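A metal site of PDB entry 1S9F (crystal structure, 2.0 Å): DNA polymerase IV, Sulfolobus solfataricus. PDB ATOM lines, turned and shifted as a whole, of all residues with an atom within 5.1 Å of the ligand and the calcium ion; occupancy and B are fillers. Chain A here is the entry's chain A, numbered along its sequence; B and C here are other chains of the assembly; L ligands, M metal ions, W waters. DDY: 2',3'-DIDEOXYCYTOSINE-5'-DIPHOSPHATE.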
ATOM      1  N   ASP A   7      24.276  10.355  16.129  1.00  0.00           N
ATOM      2  CA  ASP A   7      22.883  10.619  16.448  1.00  0.00           C
ATOM      3  C   ASP A   7      22.370  11.751  15.556  1.00  0.00           C
ATOM      4  O   ASP A   7      22.741  12.912  15.743  1.00  0.00           O
ATOM      5  CB  ASP A   7      22.822  10.964  17.940  1.00  0.00           C
ATOM      6  CG  ASP A   7      21.454  11.397  18.410  1.00  0.00           C
ATOM      7  OD1 ASP A   7      21.096  11.093  19.565  1.00  0.00           O
ATOM      8  OD2 ASP A   7      20.758  12.048  17.621  1.00  0.00           O
ATOM      9  N   PHE A   8      21.519  11.431  14.574  1.00  0.00           N
ATOM     10  CA  PHE A   8      20.994  12.430  13.641  1.00  0.00           C
ATOM     11  C   PHE A   8      20.204  13.511  14.392  1.00  0.00           C
ATOM     12  O   PHE A   8      19.412  13.177  15.254  1.00  0.00           O
ATOM     13  CB  PHE A   8      20.094  11.771  12.582  1.00  0.00           C
ATOM     14  CG  PHE A   8      20.670  10.526  11.953  1.00  0.00           C
ATOM     15  CD1 PHE A   8      22.039  10.228  12.067  1.00  0.00           C
ATOM     16  CD2 PHE A   8      19.852   9.659  11.238  1.00  0.00           C
ATOM     17  CE1 PHE A   8      22.572   9.071  11.478  1.00  0.00           C
ATOM     18  CE2 PHE A   8      20.375   8.502  10.649  1.00  0.00           C
ATOM     19  CZ  PHE A   8      21.744   8.204  10.763  1.00  0.00           C
ATOM     20  N   ASP A   9      20.385  14.788  14.049  1.00  0.00           N
ATOM     21  CA  ASP A   9      19.674  15.861  14.759  1.00  0.00           C
ATOM     22  C   ASP A   9      18.181  16.001  14.391  1.00  0.00           C
ATOM     23  O   ASP A   9      17.830  16.003  13.205  1.00  0.00           O
ATOM     24  CB  ASP A   9      20.392  17.201  14.522  1.00  0.00           C
ATOM     25  CG  ASP A   9      21.864  17.158  14.922  1.00  0.00           C
ATOM     26  OD1 ASP A   9      22.184  16.569  15.984  1.00  0.00           O
ATOM     27  OD2 ASP A   9      22.706  17.726  14.185  1.00  0.00           O
ATOM     28  N   TYR A  10      17.307  16.114  15.404  1.00  0.00           N
ATOM     29  CA  TYR A  10      15.852  16.240  15.219  1.00  0.00           C
ATOM     30  C   TYR A  10      15.428  15.622  13.891  1.00  0.00           C
ATOM     31  O   TYR A  10      14.719  16.240  13.073  1.00  0.00           O
ATOM     32  CB  TYR A  10      15.440  17.739  15.303  1.00  0.00           C
ATOM     33  CG  TYR A  10      16.063  18.673  14.265  1.00  0.00           C
ATOM     34  CD1 TYR A  10      15.304  19.173  13.215  1.00  0.00           C
ATOM     35  CD2 TYR A  10      17.401  19.053  14.348  1.00  0.00           C
ATOM     36  CE1 TYR A  10      15.861  20.039  12.273  1.00  0.00           C
ATOM     37  CE2 TYR A  10      17.978  19.917  13.406  1.00  0.00           C
ATOM     38  CZ  TYR A  10      17.188  20.406  12.373  1.00  0.00           C
ATOM     39  OH  TYR A  10      17.724  21.265  11.429  1.00  0.00           O
ATOM     40  N   PHE A  11      15.851  14.361  13.707  1.00  0.00           N
ATOM     41  CA  PHE A  11      15.699  13.639  12.464  1.00  0.00           C
ATOM     42  C   PHE A  11      14.488  13.792  11.572  1.00  0.00           C
ATOM     43  O   PHE A  11      14.638  14.244  10.436  1.00  0.00           O
ATOM     44  CB  PHE A  11      16.003  12.158  12.659  1.00  0.00           C
ATOM     45  CG  PHE A  11      16.250  11.412  11.367  1.00  0.00           C
ATOM     46  CD1 PHE A  11      17.110  11.947  10.408  1.00  0.00           C
ATOM     47  CD2 PHE A  11      15.585  10.226  11.086  1.00  0.00           C
ATOM     48  CE1 PHE A  11      17.316  11.311   9.192  1.00  0.00           C
ATOM     49  CE2 PHE A  11      15.780   9.572   9.865  1.00  0.00           C
ATOM     50  CZ  PHE A  11      16.651  10.116   8.908  1.00  0.00           C
ATOM     51  N   TYR A  12      13.310  13.400  12.024  1.00  0.00           N
ATOM     52  CA  TYR A  12      12.146  13.515  11.145  1.00  0.00           C
ATOM     53  C   TYR A  12      11.918  14.939  10.672  1.00  0.00           C
ATOM     54  O   TYR A  12      11.699  15.188   9.483  1.00  0.00           O
ATOM     55  CB  TYR A  12      10.878  13.014  11.837  1.00  0.00           C
ATOM     56  CG  TYR A  12      10.912  11.557  12.256  1.00  0.00           C
ATOM     57  CD1 TYR A  12      11.923  10.708  11.808  1.00  0.00           C
ATOM     58  CD2 TYR A  12       9.913  11.033  13.082  1.00  0.00           C
ATOM     59  CE1 TYR A  12      11.937   9.370  12.162  1.00  0.00           C
ATOM     60  CE2 TYR A  12       9.927   9.694  13.446  1.00  0.00           C
ATOM     61  CZ  TYR A  12      10.940   8.866  12.992  1.00  0.00           C
ATOM     62  OH  TYR A  12      10.977   7.551  13.372  1.00  0.00           O
ATOM     63  N   VAL A  43       3.065  14.299  19.189  1.00  0.00           N
ATOM     64  CA  VAL A  43       4.206  14.840  18.462  1.00  0.00           C
ATOM     65  C   VAL A  43       5.310  13.790  18.452  1.00  0.00           C
ATOM     66  O   VAL A  43       5.675  13.253  19.497  1.00  0.00           O
ATOM     67  CB  VAL A  43       4.730  16.137  19.166  1.00  0.00           C
ATOM     68  CG1 VAL A  43       6.016  16.610  18.499  1.00  0.00           C
ATOM     69  CG2 VAL A  43       3.671  17.246  19.129  1.00  0.00           C
ATOM     70  N   ALA A  44       5.835  13.468  17.272  1.00  0.00           N
ATOM     71  CA  ALA A  44       6.925  12.490  17.176  1.00  0.00           C
ATOM     72  C   ALA A  44       8.222  13.214  17.478  1.00  0.00           C
ATOM     73  O   ALA A  44       9.092  12.717  18.204  1.00  0.00           O
ATOM     74  CB  ALA A  44       6.972  11.870  15.765  1.00  0.00           C
ATOM     75  N   THR A  45       8.365  14.404  16.899  1.00  0.00           N
ATOM     76  CA  THR A  45       9.513  15.262  17.126  1.00  0.00           C
ATOM     77  C   THR A  45       9.272  16.643  16.531  1.00  0.00           C
ATOM     78  O   THR A  45       8.357  16.859  15.751  1.00  0.00           O
ATOM     79  CB  THR A  45      10.819  14.688  16.531  1.00  0.00           C
ATOM     80  OG1 THR A  45      11.906  15.535  16.918  1.00  0.00           O
ATOM     81  CG2 THR A  45      10.755  14.629  15.009  1.00  0.00           C
ATOM     82  N   ALA A  46      10.106  17.593  16.927  1.00  0.00           N
ATOM     83  CA  ALA A  46       9.994  18.958  16.443  1.00  0.00           C
ATOM     84  C   ALA A  46      11.398  19.524  16.271  1.00  0.00           C
ATOM     85  O   ALA A  46      12.322  19.074  16.947  1.00  0.00           O
ATOM     86  CB  ALA A  46       9.222  19.785  17.445  1.00  0.00           C
ATOM     87  N   TYR A  48      14.444  22.370  16.586  1.00  0.00           N
ATOM     88  CA  TYR A  48      14.819  23.116  17.777  1.00  0.00           C
ATOM     89  C   TYR A  48      14.111  24.445  17.951  1.00  0.00           C
ATOM     90  O   TYR A  48      13.992  24.932  19.064  1.00  0.00           O
ATOM     91  CB  TYR A  48      16.339  23.274  17.864  1.00  0.00           C
ATOM     92  CG  TYR A  48      17.022  22.011  18.362  1.00  0.00           C
ATOM     93  CD1 TYR A  48      17.208  20.907  17.531  1.00  0.00           C
ATOM     94  CD2 TYR A  48      17.455  21.917  19.692  1.00  0.00           C
ATOM     95  CE1 TYR A  48      17.808  19.729  18.005  1.00  0.00           C
ATOM     96  CE2 TYR A  48      18.046  20.747  20.178  1.00  0.00           C
ATOM     97  CZ  TYR A  48      18.223  19.661  19.321  1.00  0.00           C
ATOM     98  OH  TYR A  48      18.817  18.522  19.804  1.00  0.00           O
ATOM     99  N   ARG A  51      11.134  23.579  19.900  1.00  0.00           N
ATOM    100  CA  ARG A  51      11.476  23.131  21.241  1.00  0.00           C
ATOM    101  C   ARG A  51      11.738  24.305  22.178  1.00  0.00           C
ATOM    102  O   ARG A  51      11.567  24.200  23.381  1.00  0.00           O
ATOM    103  CB  ARG A  51      12.701  22.208  21.211  1.00  0.00           C
ATOM    104  CG  ARG A  51      12.481  20.927  20.414  1.00  0.00           C
ATOM    105  CD  ARG A  51      13.717  20.019  20.450  1.00  0.00           C
ATOM    106  NE  ARG A  51      13.624  18.942  19.476  1.00  0.00           N
ATOM    107  CZ  ARG A  51      14.446  17.884  19.428  1.00  0.00           C
ATOM    108  NH1 ARG A  51      15.429  17.762  20.312  1.00  0.00           N
ATOM    109  NH2 ARG A  51      14.278  16.972  18.480  1.00  0.00           N
ATOM    110  N   ALA A  57       8.729  15.853  21.746  1.00  0.00           N
ATOM    111  CA  ALA A  57       8.175  14.549  21.399  1.00  0.00           C
ATOM    112  C   ALA A  57       7.334  14.011  22.542  1.00  0.00           C
ATOM    113  O   ALA A  57       7.690  14.179  23.705  1.00  0.00           O
ATOM    114  CB  ALA A  57       9.305  13.575  21.089  1.00  0.00           C
ATOM    115  N   GLY A  58       6.217  13.390  22.215  1.00  0.00           N
ATOM    116  CA  GLY A  58       5.364  12.816  23.248  1.00  0.00           C
ATOM    117  C   GLY A  58       4.147  13.610  23.659  1.00  0.00           C
ATOM    118  O   GLY A  58       3.163  13.020  24.090  1.00  0.00           O
ATOM    119  N   ILE A 104      16.436   3.946  14.206  1.00  0.00           N
ATOM    120  CA  ILE A 104      16.350   4.691  12.957  1.00  0.00           C
ATOM    121  C   ILE A 104      17.344   5.849  12.829  1.00  0.00           C
ATOM    122  O   ILE A 104      17.727   6.215  11.709  1.00  0.00           O
ATOM    123  CB  ILE A 104      14.900   5.218  12.729  1.00  0.00           C
ATOM    124  CG1 ILE A 104      14.753   5.713  11.290  1.00  0.00           C
ATOM    125  CG2 ILE A 104      14.572   6.303  13.737  1.00  0.00           C
ATOM    126  CD1 ILE A 104      13.306   5.914  10.865  1.00  0.00           C
ATOM    127  N   ASP A 105      17.775   6.435  13.934  1.00  0.00           N
ATOM    128  CA  ASP A 105      18.705   7.547  13.804  1.00  0.00           C
ATOM    129  C   ASP A 105      19.888   7.544  14.770  1.00  0.00           C
ATOM    130  O   ASP A 105      20.432   8.605  15.103  1.00  0.00           O
ATOM    131  CB  ASP A 105      17.936   8.867  13.902  1.00  0.00           C
ATOM    132  CG  ASP A 105      17.722   9.304  15.319  1.00  0.00           C
ATOM    133  OD1 ASP A 105      17.458   8.467  16.202  1.00  0.00           O
ATOM    134  OD2 ASP A 105      17.827  10.522  15.535  1.00  0.00           O
ATOM    135  N   LYS A 159      24.517  17.586  21.347  1.00  0.00           N
ATOM    136  CA  LYS A 159      23.508  17.872  20.335  1.00  0.00           C
ATOM    137  C   LYS A 159      22.864  19.244  20.520  1.00  0.00           C
ATOM    138  O   LYS A 159      22.767  19.747  21.647  1.00  0.00           O
ATOM    139  CB  LYS A 159      22.439  16.763  20.279  1.00  0.00           C
ATOM    140  CG  LYS A 159      21.618  16.567  21.541  1.00  0.00           C
ATOM    141  CD  LYS A 159      20.540  15.473  21.374  1.00  0.00           C
ATOM    142  CE  LYS A 159      21.166  14.115  20.998  1.00  0.00           C
ATOM    143  NZ  LYS A 159      20.166  12.997  21.002  1.00  0.00           N
ATOM    144  P    DG B   5      -2.448   7.669  22.194  1.00  0.00           P
ATOM    145  OP1  DG B   5      -3.844   7.892  21.744  1.00  0.00           O
ATOM    146  OP2  DG B   5      -2.061   6.345  22.753  1.00  0.00           O
ATOM    147  O5'  DG B   5      -1.495   8.010  20.967  1.00  0.00           O
ATOM    148  C5'  DG B   5      -1.957   8.810  19.888  1.00  0.00           C
ATOM    149  C4'  DG B   5      -1.171   8.491  18.642  1.00  0.00           C
ATOM    150  O4'  DG B   5       0.185   8.964  18.807  1.00  0.00           O
ATOM    151  C3'  DG B   5      -1.069   6.996  18.388  1.00  0.00           C
ATOM    152  O3'  DG B   5      -1.076   6.783  16.976  1.00  0.00           O
ATOM    153  C2'  DG B   5       0.263   6.615  19.016  1.00  0.00           C
ATOM    154  C1'  DG B   5       1.094   7.873  18.825  1.00  0.00           C
ATOM    155  N9   DG B   5       2.072   8.159  19.863  1.00  0.00           N
ATOM    156  C8   DG B   5       1.837   8.346  21.213  1.00  0.00           C
ATOM    157  N7   DG B   5       2.908   8.667  21.881  1.00  0.00           N
ATOM    158  C5   DG B   5       3.914   8.693  20.933  1.00  0.00           C
ATOM    159  C6   DG B   5       5.296   8.998  21.060  1.00  0.00           C
ATOM    160  O6   DG B   5       5.926   9.333  22.061  1.00  0.00           O
ATOM    161  N1   DG B   5       5.960   8.889  19.839  1.00  0.00           N
ATOM    162  C2   DG B   5       5.377   8.531  18.649  1.00  0.00           C
ATOM    163  N2   DG B   5       6.188   8.498  17.582  1.00  0.00           N
ATOM    164  N3   DG B   5       4.087   8.240  18.517  1.00  0.00           N
ATOM    165  C4   DG B   5       3.424   8.350  19.687  1.00  0.00           C
ATOM    166  P    DT B   6      -1.274   5.305  16.402  1.00  0.00           P
ATOM    167  OP1  DT B   6      -1.810   5.479  15.026  1.00  0.00           O
ATOM    168  OP2  DT B   6      -2.018   4.485  17.391  1.00  0.00           O
ATOM    169  O5'  DT B   6       0.216   4.776  16.261  1.00  0.00           O
ATOM    170  C5'  DT B   6       1.071   5.375  15.296  1.00  0.00           C
ATOM    171  C4'  DT B   6       2.467   4.797  15.358  1.00  0.00           C
ATOM    172  O4'  DT B   6       3.224   5.319  16.486  1.00  0.00           O
ATOM    173  C3'  DT B   6       2.586   3.281  15.418  1.00  0.00           C
ATOM    174  O3'  DT B   6       3.519   2.915  14.410  1.00  0.00           O
ATOM    175  C2'  DT B   6       3.165   3.020  16.796  1.00  0.00           C
ATOM    176  C1'  DT B   6       4.006   4.269  17.002  1.00  0.00           C
ATOM    177  N1   DT B   6       4.377   4.621  18.392  1.00  0.00           N
ATOM    178  C2   DT B   6       5.684   4.992  18.615  1.00  0.00           C
ATOM    179  O2   DT B   6       6.537   4.992  17.750  1.00  0.00           O
ATOM    180  N3   DT B   6       5.966   5.364  19.904  1.00  0.00           N
ATOM    181  C4   DT B   6       5.094   5.382  20.967  1.00  0.00           C
ATOM    182  O4   DT B   6       5.488   5.767  22.067  1.00  0.00           O
ATOM    183  C5   DT B   6       3.742   4.957  20.680  1.00  0.00           C
ATOM    184  C7   DT B   6       2.734   4.918  21.779  1.00  0.00           C
ATOM    185  C6   DT B   6       3.451   4.602  19.415  1.00  0.00           C
ATOM    186  P    DA C  13      17.314   7.431  23.112  1.00  0.00           P
ATOM    187  OP1  DA C  13      18.675   7.960  22.848  1.00  0.00           O
ATOM    188  OP2  DA C  13      16.387   8.200  23.974  1.00  0.00           O
ATOM    189  O5'  DA C  13      16.597   7.141  21.719  1.00  0.00           O
ATOM    190  C5'  DA C  13      16.972   6.010  20.938  1.00  0.00           C
ATOM    191  C4'  DA C  13      15.988   5.774  19.819  1.00  0.00           C
ATOM    192  O4'  DA C  13      14.690   5.391  20.362  1.00  0.00           O
ATOM    193  C3'  DA C  13      15.720   6.955  18.891  1.00  0.00           C
ATOM    194  O3'  DA C  13      15.316   6.460  17.602  1.00  0.00           O
ATOM    195  C2'  DA C  13      14.412   7.511  19.431  1.00  0.00           C
ATOM    196  C1'  DA C  13      13.698   6.219  19.771  1.00  0.00           C
ATOM    197  N9   DA C  13      12.597   6.374  20.727  1.00  0.00           N
ATOM    198  C8   DA C  13      12.645   6.825  22.030  1.00  0.00           C
ATOM    199  N7   DA C  13      11.466   6.890  22.595  1.00  0.00           N
ATOM    200  C5   DA C  13      10.596   6.457  21.618  1.00  0.00           C
ATOM    201  C6   DA C  13       9.200   6.327  21.591  1.00  0.00           C
ATOM    202  N6   DA C  13       8.403   6.635  22.619  1.00  0.00           N
ATOM    203  N1   DA C  13       8.629   5.864  20.450  1.00  0.00           N
ATOM    204  C2   DA C  13       9.427   5.568  19.415  1.00  0.00           C
ATOM    205  N3   DA C  13      10.750   5.661  19.319  1.00  0.00           N
ATOM    206  C4   DA C  13      11.281   6.127  20.460  1.00  0.00           C
HETATM  207  C4  DDY L   1       9.657   9.872  20.946  1.00  0.00           C
HETATM  208  PB  DDY L   1      16.691  14.017  19.737  1.00  0.00           P
HETATM  209  PA  DDY L   1      15.142  13.260  17.412  1.00  0.00           P
HETATM  210  C2  DDY L   1       9.549   9.298  18.579  1.00  0.00           C
HETATM  211  C5  DDY L   1      11.003  10.230  20.808  1.00  0.00           C
HETATM  212  O2  DDY L   1       8.893   8.905  17.615  1.00  0.00           O
HETATM  213  O3B DDY L   1      16.510  15.521  19.212  1.00  0.00           O
HETATM  214  O1B DDY L   1      18.017  13.564  19.282  1.00  0.00           O
HETATM  215  O2B DDY L   1      16.407  13.990  21.182  1.00  0.00           O
HETATM  216  O3A DDY L   1      15.496  13.188  18.993  1.00  0.00           O
HETATM  217  O1A DDY L   1      16.355  13.241  16.582  1.00  0.00           O
HETATM  218  O2A DDY L   1      14.194  14.377  17.205  1.00  0.00           O
HETATM  219  O5' DDY L   1      14.340  11.879  17.228  1.00  0.00           O
HETATM  220  C5' DDY L   1      14.755  10.868  16.310  1.00  0.00           C
HETATM  221  C4' DDY L   1      13.561   9.943  16.036  1.00  0.00           C
HETATM  222  O4' DDY L   1      13.056   9.339  17.253  1.00  0.00           O
HETATM  223  C3' DDY L   1      12.530  10.677  15.597  1.00  0.00           C
HETATM  224  C2' DDY L   1      11.420  10.381  16.236  1.00  0.00           C
HETATM  225  C1' DDY L   1      11.608   9.420  17.130  1.00  0.00           C
HETATM  226  N1  DDY L   1      10.914   9.645  18.438  1.00  0.00           N
HETATM  227  C6  DDY L   1      11.637  10.118  19.565  1.00  0.00           C
HETATM  228  N4  DDY L   1       9.062   9.962  22.133  1.00  0.00           N
HETATM  229  N3  DDY L   1       8.936   9.413  19.843  1.00  0.00           N
HETATM  230 CA    CA M   1      18.367  12.253  17.219  1.00  0.00          CA
HETATM  231  O   HOH W   1      17.923  10.145  18.826  1.00  0.00           O
HETATM  232  O   HOH W   2      10.547  11.012  24.277  1.00  0.00           O
HETATM  233  O   HOH W   3      18.637  16.425  17.870  1.00  0.00           O
HETATM  234  O   HOH W   4      12.278  14.052  19.133  1.00  0.00           O
HETATM  235  O   HOH W   5       9.433   7.009  15.434  1.00  0.00           O
HETATM  236  O   HOH W   6      13.515  13.623  21.359  1.00  0.00           O
HETATM  237  O   HOH W   7      16.827  15.490  23.159  1.00  0.00           O
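An oxygen (O2A) of the ligand lies within hydrogen-bond range of the side-chain hydroxyl of Thr 45, at 2.6 Å.
The backbone NH (N) of Tyr 10 lies close to an oxygen (O1A) of the ligand, 3.2 Å away.
The backbone NH (N) of Phe 11 lies close to an oxygen (O1A) of the ligand, 3.1 Å away.
N4 of the ligand is in hydrogen-bond range of O6 of DG 5 of chain B.
N6 of DA 13 of chain C lies within hydrogen-bond range of N4 of the ligand, at 3.4 Å.
An oxygen (O2B) of the ligand is in salt-bridge range of the side-chain amino group (NZ) of Lys 159 (3.9 Å).
NH1 of Arg 51 is in salt-bridge range of O3B of the ligand.
The guanidinium group (NE) of Arg 51 sits at hydrogen-bond distance from the backbone carbonyl oxygen (O) of Ala 46 (2.8 Å).
The side-chain carboxylate of Asp 7 is in salt-bridge range of the side-chain amino group of Lys 159 (2.6 Å).
The side-chain hydroxyl of Thr 45 is in hydrogen-bond range of the guanidinium group of Arg 51, at 3.2 Å.
Merely in contact with the ligand: Asp 9 (3.97 Å), Tyr 12 (3.2 Å), Ala 44 (3.5 Å), Tyr 48 (3.8 Å) and Ala 57 (3.7 Å).
Hydrophobic or aromatic side chains within 4 Å of the ligand: Tyr 12, Ala 44 and Ala 57.
The nearest printed residue that does not touch the ligand is Ile 104 (4.4 Å).
Of the 20 residues printed, 3 come within 4 Å of the calcium ion.
The calcium ion is bound by O1A of the ligand (2.3 Å), O of Phe 8 (2.4 Å), OD2 of Asp 7 (2.4 Å), O1B of the ligand (2.5 Å), OD2 of Asp 105 (2.5 Å) and water W1 (2.7 Å).
Water W1 bridges the side-chain carboxylate of Asp 105 and the side-chain carboxylate of Asp 7.
Water W3 lies within hydrogen-bond range of O3B of the ligand (2.7 Å), N of Tyr 10 (2.8 Å) and OH of Tyr 48 (2.9 Å).
Water W4 bridges OG1 of Thr 45 and O2A of the ligand.
Water W5 bridges the side-chain hydroxyl (OH) of Tyr 12 (2.6 Å) and an oxygen (O2) of the ligand (2.9 Å).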
